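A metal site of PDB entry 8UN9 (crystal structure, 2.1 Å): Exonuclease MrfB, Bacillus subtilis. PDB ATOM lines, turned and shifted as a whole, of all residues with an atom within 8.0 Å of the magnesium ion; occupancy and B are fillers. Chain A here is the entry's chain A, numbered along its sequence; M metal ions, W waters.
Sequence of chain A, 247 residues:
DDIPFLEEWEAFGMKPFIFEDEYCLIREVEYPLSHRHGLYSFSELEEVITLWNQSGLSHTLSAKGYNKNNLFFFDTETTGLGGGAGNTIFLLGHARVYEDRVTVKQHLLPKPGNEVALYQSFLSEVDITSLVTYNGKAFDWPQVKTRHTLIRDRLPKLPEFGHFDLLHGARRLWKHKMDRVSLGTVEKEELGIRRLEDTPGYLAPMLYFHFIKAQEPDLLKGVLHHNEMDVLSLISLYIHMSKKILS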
ATOM      1  N   PHE A  74      -0.703  -1.215   0.227  1.00  0.00           N
ATOM      2  CA  PHE A  74      -1.269   0.122   0.127  1.00  0.00           C
ATOM      3  C   PHE A  74      -0.153   1.157   0.205  1.00  0.00           C
ATOM      4  O   PHE A  74       0.628   1.168   1.166  1.00  0.00           O
ATOM      5  CB  PHE A  74      -2.271   0.316   1.268  1.00  0.00           C
ATOM      6  CG  PHE A  74      -2.893   1.682   1.361  1.00  0.00           C
ATOM      7  CD1 PHE A  74      -3.751   2.158   0.372  1.00  0.00           C
ATOM      8  CD2 PHE A  74      -2.654   2.503   2.456  1.00  0.00           C
ATOM      9  CE1 PHE A  74      -4.323   3.407   0.469  1.00  0.00           C
ATOM     10  CE2 PHE A  74      -3.223   3.763   2.540  1.00  0.00           C
ATOM     11  CZ  PHE A  74      -4.059   4.216   1.551  1.00  0.00           C
ATOM     12  N   ASP A  75      -0.173   2.126  -0.729  1.00  0.00           N
ATOM     13  CA  ASP A  75       0.765   3.243  -0.695  1.00  0.00           C
ATOM     14  C   ASP A  75       0.101   4.490  -1.248  1.00  0.00           C
ATOM     15  O   ASP A  75      -0.717   4.392  -2.180  1.00  0.00           O
ATOM     16  CB  ASP A  75       2.015   2.872  -1.502  1.00  0.00           C
ATOM     17  CG  ASP A  75       3.065   3.964  -1.477  1.00  0.00           C
ATOM     18  OD1 ASP A  75       3.664   4.146  -0.417  1.00  0.00           O
ATOM     19  OD2 ASP A  75       3.189   4.689  -2.508  1.00  0.00           O
ATOM     20  N   THR A  76       0.455   5.661  -0.697  1.00  0.00           N
ATOM     21  CA  THR A  76      -0.211   6.920  -0.997  1.00  0.00           C
ATOM     22  C   THR A  76       0.806   7.958  -1.434  1.00  0.00           C
ATOM     23  O   THR A  76       1.964   7.870  -1.087  1.00  0.00           O
ATOM     24  CB  THR A  76      -1.011   7.466   0.176  1.00  0.00           C
ATOM     25  OG1 THR A  76      -0.109   7.882   1.200  1.00  0.00           O
ATOM     26  CG2 THR A  76      -1.990   6.476   0.767  1.00  0.00           C
ATOM     27  N   GLU A  77       0.356   8.951  -2.215  1.00  0.00           N
ATOM     28  CA  GLU A  77       1.154  10.137  -2.436  1.00  0.00           C
ATOM     29  C   GLU A  77       0.351  11.318  -1.887  1.00  0.00           C
ATOM     30  O   GLU A  77      -0.891  11.284  -1.885  1.00  0.00           O
ATOM     31  CB  GLU A  77       1.490  10.297  -3.908  1.00  0.00           C
ATOM     32  CG  GLU A  77       2.162   9.093  -4.554  1.00  0.00           C
ATOM     33  CD  GLU A  77       3.449   8.606  -3.894  1.00  0.00           C
ATOM     34  OE1 GLU A  77       4.219   9.480  -3.447  1.00  0.00           O
ATOM     35  OE2 GLU A  77       3.651   7.367  -3.809  1.00  0.00           O
ATOM     36  N   THR A  78       1.067  12.355  -1.439  1.00  0.00           N
ATOM     37  CA  THR A  78       0.495  13.483  -0.726  1.00  0.00           C
ATOM     38  C   THR A  78       0.984  14.789  -1.320  1.00  0.00           C
ATOM     39  O   THR A  78       1.930  14.793  -2.107  1.00  0.00           O
ATOM     40  CB  THR A  78       0.869  13.464   0.764  1.00  0.00           C
ATOM     41  OG1 THR A  78       2.289  13.544   0.862  1.00  0.00           O
ATOM     42  CG2 THR A  78       0.401  12.220   1.483  1.00  0.00           C
ATOM     43  N   LEU A  91      -3.453  10.630  -3.877  1.00  0.00           N
ATOM     44  CA  LEU A  91      -3.436   9.389  -4.634  1.00  0.00           C
ATOM     45  C   LEU A  91      -3.423   8.207  -3.668  1.00  0.00           C
ATOM     46  O   LEU A  91      -2.547   8.092  -2.807  1.00  0.00           O
ATOM     47  CB  LEU A  91      -2.234   9.397  -5.579  1.00  0.00           C
ATOM     48  CG  LEU A  91      -1.995   8.120  -6.384  1.00  0.00           C
ATOM     49  CD1 LEU A  91      -3.159   7.850  -7.340  1.00  0.00           C
ATOM     50  CD2 LEU A  91      -0.678   8.198  -7.175  1.00  0.00           C
ATOM     51  N   TYR A 134       4.355   0.667   4.147  1.00  0.00           N
ATOM     52  CA  TYR A 134       5.698   1.143   4.426  1.00  0.00           C
ATOM     53  C   TYR A 134       5.609   2.665   4.515  1.00  0.00           C
ATOM     54  O   TYR A 134       6.084   3.331   3.623  1.00  0.00           O
ATOM     55  CB  TYR A 134       6.635   0.694   3.296  1.00  0.00           C
ATOM     56  CG  TYR A 134       8.131   0.775   3.592  1.00  0.00           C
ATOM     57  CD1 TYR A 134       8.727  -0.222   4.332  1.00  0.00           C
ATOM     58  CD2 TYR A 134       8.920   1.871   3.226  1.00  0.00           C
ATOM     59  CE1 TYR A 134      10.087  -0.172   4.671  1.00  0.00           C
ATOM     60  CE2 TYR A 134      10.275   1.925   3.552  1.00  0.00           C
ATOM     61  CZ  TYR A 134      10.866   0.888   4.260  1.00  0.00           C
ATOM     62  OH  TYR A 134      12.184   0.828   4.624  1.00  0.00           O
ATOM     63  N   LEU A 183      12.406   3.460   0.759  1.00  0.00           N
ATOM     64  CA  LEU A 183      11.950   2.320  -0.049  1.00  0.00           C
ATOM     65  C   LEU A 183      12.916   2.074  -1.214  1.00  0.00           C
ATOM     66  O   LEU A 183      13.231   0.926  -1.507  1.00  0.00           O
ATOM     67  CB  LEU A 183      10.512   2.523  -0.548  1.00  0.00           C
ATOM     68  CG  LEU A 183       9.847   1.317  -1.233  1.00  0.00           C
ATOM     69  CD1 LEU A 183       9.856   0.075  -0.367  1.00  0.00           C
ATOM     70  CD2 LEU A 183       8.398   1.624  -1.638  1.00  0.00           C
ATOM     71  N   ARG A 195      14.502   0.720 -10.875  1.00  0.00           N
ATOM     72  CA  ARG A 195      13.447   1.439 -11.577  1.00  0.00           C
ATOM     73  C   ARG A 195      14.072   2.199 -12.742  1.00  0.00           C
ATOM     74  O   ARG A 195      15.165   2.735 -12.601  1.00  0.00           O
ATOM     75  CB  ARG A 195      12.755   2.425 -10.654  1.00  0.00           C
ATOM     76  CG  ARG A 195      12.057   1.807  -9.463  1.00  0.00           C
ATOM     77  CD  ARG A 195      11.256   2.879  -8.741  1.00  0.00           C
ATOM     78  NE  ARG A 195      10.667   2.381  -7.520  1.00  0.00           N
ATOM     79  CZ  ARG A 195       9.529   2.772  -6.983  1.00  0.00           C
ATOM     80  NH1 ARG A 195       8.881   3.815  -7.481  1.00  0.00           N
ATOM     81  NH2 ARG A 195       9.053   2.137  -5.919  1.00  0.00           N
ATOM     82  N   THR A 199       9.965   8.846 -11.424  1.00  0.00           N
ATOM     83  CA  THR A 199       9.621  10.155 -10.898  1.00  0.00           C
ATOM     84  C   THR A 199       9.568  10.074  -9.388  1.00  0.00           C
ATOM     85  O   THR A 199       8.716   9.405  -8.814  1.00  0.00           O
ATOM     86  CB  THR A 199       8.266  10.636 -11.433  1.00  0.00           C
ATOM     87  OG1 THR A 199       8.365  10.724 -12.850  1.00  0.00           O
ATOM     88  CG2 THR A 199       7.894  11.978 -10.849  1.00  0.00           C
ATOM     89  N   PRO A 200      10.500  10.723  -8.665  1.00  0.00           N
ATOM     90  CA  PRO A 200      10.601  10.516  -7.230  1.00  0.00           C
ATOM     91  C   PRO A 200       9.406  11.104  -6.511  1.00  0.00           C
ATOM     92  O   PRO A 200       8.788  12.065  -6.987  1.00  0.00           O
ATOM     93  CB  PRO A 200      11.906  11.224  -6.796  1.00  0.00           C
ATOM     94  CG  PRO A 200      12.573  11.683  -8.073  1.00  0.00           C
ATOM     95  CD  PRO A 200      11.561  11.586  -9.188  1.00  0.00           C
ATOM     96  N   GLY A 201       9.121  10.519  -5.335  1.00  0.00           N
ATOM     97  CA  GLY A 201       7.961  10.887  -4.539  1.00  0.00           C
ATOM     98  C   GLY A 201       7.970  12.346  -4.131  1.00  0.00           C
ATOM     99  O   GLY A 201       6.914  12.965  -4.150  1.00  0.00           O
ATOM    100  N   TYR A 202       9.155  12.882  -3.799  1.00  0.00           N
ATOM    101  CA  TYR A 202       9.277  14.261  -3.384  1.00  0.00           C
ATOM    102  C   TYR A 202       8.924  15.223  -4.530  1.00  0.00           C
ATOM    103  O   TYR A 202       8.801  16.420  -4.273  1.00  0.00           O
ATOM    104  CB  TYR A 202      10.649  14.523  -2.744  1.00  0.00           C
ATOM    105  CG  TYR A 202      11.858  14.145  -3.600  1.00  0.00           C
ATOM    106  CD1 TYR A 202      12.268  14.968  -4.651  1.00  0.00           C
ATOM    107  CD2 TYR A 202      12.570  12.972  -3.380  1.00  0.00           C
ATOM    108  CE1 TYR A 202      13.353  14.632  -5.441  1.00  0.00           C
ATOM    109  CE2 TYR A 202      13.685  12.650  -4.146  1.00  0.00           C
ATOM    110  CZ  TYR A 202      14.064  13.478  -5.184  1.00  0.00           C
ATOM    111  OH  TYR A 202      15.109  13.192  -5.976  1.00  0.00           O
ATOM    112  N   ALA A 204       6.058  14.708  -6.354  1.00  0.00           N
ATOM    113  CA  ALA A 204       4.623  14.550  -6.537  1.00  0.00           C
ATOM    114  C   ALA A 204       3.874  15.809  -6.097  1.00  0.00           C
ATOM    115  O   ALA A 204       3.002  16.265  -6.837  1.00  0.00           O
ATOM    116  CB  ALA A 204       4.125  13.325  -5.778  1.00  0.00           C
ATOM    117  N   VAL A 223       4.144  10.118 -11.791  1.00  0.00           N
ATOM    118  CA  VAL A 223       3.762   9.938 -10.408  1.00  0.00           C
ATOM    119  C   VAL A 223       2.980   8.633 -10.264  1.00  0.00           C
ATOM    120  O   VAL A 223       3.153   7.881  -9.298  1.00  0.00           O
ATOM    121  CB  VAL A 223       2.949  11.139  -9.889  1.00  0.00           C
ATOM    122  CG1 VAL A 223       2.365  10.874  -8.514  1.00  0.00           C
ATOM    123  CG2 VAL A 223       3.764  12.426  -9.902  1.00  0.00           C
ATOM    124  N   HIS A 226       5.205   5.694 -10.480  1.00  0.00           N
ATOM    125  CA  HIS A 226       6.026   5.594  -9.283  1.00  0.00           C
ATOM    126  C   HIS A 226       5.229   4.895  -8.184  1.00  0.00           C
ATOM    127  O   HIS A 226       5.736   3.987  -7.535  1.00  0.00           O
ATOM    128  CB  HIS A 226       6.521   6.988  -8.897  1.00  0.00           C
ATOM    129  CG  HIS A 226       7.038   7.059  -7.499  1.00  0.00           C
ATOM    130  ND1 HIS A 226       8.360   6.910  -7.160  1.00  0.00           N
ATOM    131  CD2 HIS A 226       6.360   7.263  -6.354  1.00  0.00           C
ATOM    132  CE1 HIS A 226       8.459   7.027  -5.826  1.00  0.00           C
ATOM    133  NE2 HIS A 226       7.253   7.230  -5.322  1.00  0.00           N
ATOM    134  N   ASN A 227       3.963   5.289  -8.020  1.00  0.00           N
ATOM    135  CA  ASN A 227       3.089   4.751  -7.021  1.00  0.00           C
ATOM    136  C   ASN A 227       2.765   3.286  -7.304  1.00  0.00           C
ATOM    137  O   ASN A 227       2.683   2.499  -6.352  1.00  0.00           O
ATOM    138  CB  ASN A 227       1.847   5.619  -6.879  1.00  0.00           C
ATOM    139  CG  ASN A 227       0.833   5.027  -5.958  1.00  0.00           C
ATOM    140  OD1 ASN A 227      -0.125   4.401  -6.416  1.00  0.00           O
ATOM    141  ND2 ASN A 227       1.008   5.221  -4.664  1.00  0.00           N
ATOM    142  N   GLU A 228       2.588   2.957  -8.579  1.00  0.00           N
ATOM    143  CA  GLU A 228       2.373   1.593  -9.040  1.00  0.00           C
ATOM    144  C   GLU A 228       3.579   0.741  -8.649  1.00  0.00           C
ATOM    145  O   GLU A 228       3.424  -0.380  -8.155  1.00  0.00           O
ATOM    146  CB  GLU A 228       2.166   1.588 -10.560  1.00  0.00           C
ATOM    147  CG  GLU A 228       1.952   0.233 -11.206  1.00  0.00           C
ATOM    148  CD  GLU A 228       1.821   0.294 -12.730  1.00  0.00           C
ATOM    149  OE1 GLU A 228       1.693   1.430 -13.291  1.00  0.00           O
ATOM    150  OE2 GLU A 228       1.897  -0.769 -13.369  1.00  0.00           O
ATOM    151  N   MET A 229       4.782   1.258  -8.905  1.00  0.00           N
ATOM    152  CA  MET A 229       5.994   0.519  -8.580  1.00  0.00           C
ATOM    153  C   MET A 229       6.095   0.376  -7.058  1.00  0.00           C
ATOM    154  O   MET A 229       6.400  -0.718  -6.600  1.00  0.00           O
ATOM    155  CB  MET A 229       7.248   1.180  -9.137  1.00  0.00           C
ATOM    156  CG  MET A 229       7.310   1.101 -10.639  1.00  0.00           C
ATOM    157  SD  MET A 229       7.490  -0.585 -11.234  1.00  0.00           S
ATOM    158  CE  MET A 229       9.263  -0.793 -11.066  1.00  0.00           C
ATOM    159  N   ASP A 230       5.700   1.409  -6.299  1.00  0.00           N
ATOM    160  CA  ASP A 230       5.644   1.353  -4.850  1.00  0.00           C
ATOM    161  C   ASP A 230       4.816   0.169  -4.337  1.00  0.00           C
ATOM    162  O   ASP A 230       5.301  -0.559  -3.491  1.00  0.00           O
ATOM    163  CB  ASP A 230       5.147   2.667  -4.210  1.00  0.00           C
ATOM    164  CG  ASP A 230       6.113   3.859  -4.267  1.00  0.00           C
ATOM    165  OD1 ASP A 230       7.295   3.650  -4.647  1.00  0.00           O
ATOM    166  OD2 ASP A 230       5.667   4.992  -3.999  1.00  0.00           O
ATOM    167  N   VAL A 231       3.574  -0.008  -4.824  1.00  0.00           N
ATOM    168  CA  VAL A 231       2.695  -1.013  -4.260  1.00  0.00           C
ATOM    169  C   VAL A 231       3.189  -2.410  -4.640  1.00  0.00           C
ATOM    170  O   VAL A 231       3.120  -3.302  -3.791  1.00  0.00           O
ATOM    171  CB  VAL A 231       1.186  -0.779  -4.560  1.00  0.00           C
ATOM    172  CG1 VAL A 231       0.716   0.579  -4.067  1.00  0.00           C
ATOM    173  CG2 VAL A 231       0.809  -0.918  -6.012  1.00  0.00           C
ATOM    174  N   LEU A 234       5.953  -3.349  -2.229  1.00  0.00           N
ATOM    175  CA  LEU A 234       5.444  -3.764  -0.930  1.00  0.00           C
ATOM    176  C   LEU A 234       5.169  -5.259  -0.904  1.00  0.00           C
ATOM    177  O   LEU A 234       5.312  -5.919   0.144  1.00  0.00           O
ATOM    178  CB  LEU A 234       4.167  -2.995  -0.584  1.00  0.00           C
ATOM    179  CG  LEU A 234       4.326  -1.492  -0.392  1.00  0.00           C
ATOM    180  CD1 LEU A 234       3.004  -0.841   0.002  1.00  0.00           C
ATOM    181  CD2 LEU A 234       5.397  -1.194   0.652  1.00  0.00           C
HETATM  182 MG    MG M   1       5.129   6.218  -2.518  1.00  0.00          MG
HETATM  183  O   HOH W   1       6.267   5.198  -1.234  1.00  0.00           O
HETATM  184  O   HOH W   2       6.383   7.618  -3.174  1.00  0.00           O
HETATM  185  O   HOH W   3       4.368   6.967  -0.853  1.00  0.00           O
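The side-chain carboxylate (OD2) of Asp 230 sits close to a ring nitrogen (NE2) of His 226, at 3.0 Å.
The side-chain carboxylate (OD1) of Asp 230 lies within salt-bridge range of the guanidinium group (NH2) of Arg 195 (2.6 Å).
O of Leu 91 lies within hydrogen-bond range of N of Glu 77 (3.1 Å).
O of Asp 75 sits at hydrogen-bond distance from ND2 of Asn 227 (3.1 Å).
O of His 226 lies within hydrogen-bond range of NH1 of Arg 195 (3.2 Å).
ND1 of His 226 lies within hydrogen-bond range of O of Thr 199 (3.0 Å).
Thr 76 touches the magnesium ion.
His 226 touches the magnesium ion.
The nearest printed residue that does not touch the magnesium ion is Asn 227 (4.8 Å).
The magnesium ion is bound by water W3 (2.0 Å), water W2 (2.0 Å), water W1 (2.0 Å), the side-chain carboxylate (OD2) of Asp 230 (2.0 Å), the side-chain carboxylate (OE2) of Glu 77 (2.3 Å) and the side-chain carboxylate (OD2) of Asp 75 (2.5 Å).
Water W3 bridges O of Thr 76 (2.6 Å) and OD1 of Asp 75 (2.9 Å).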
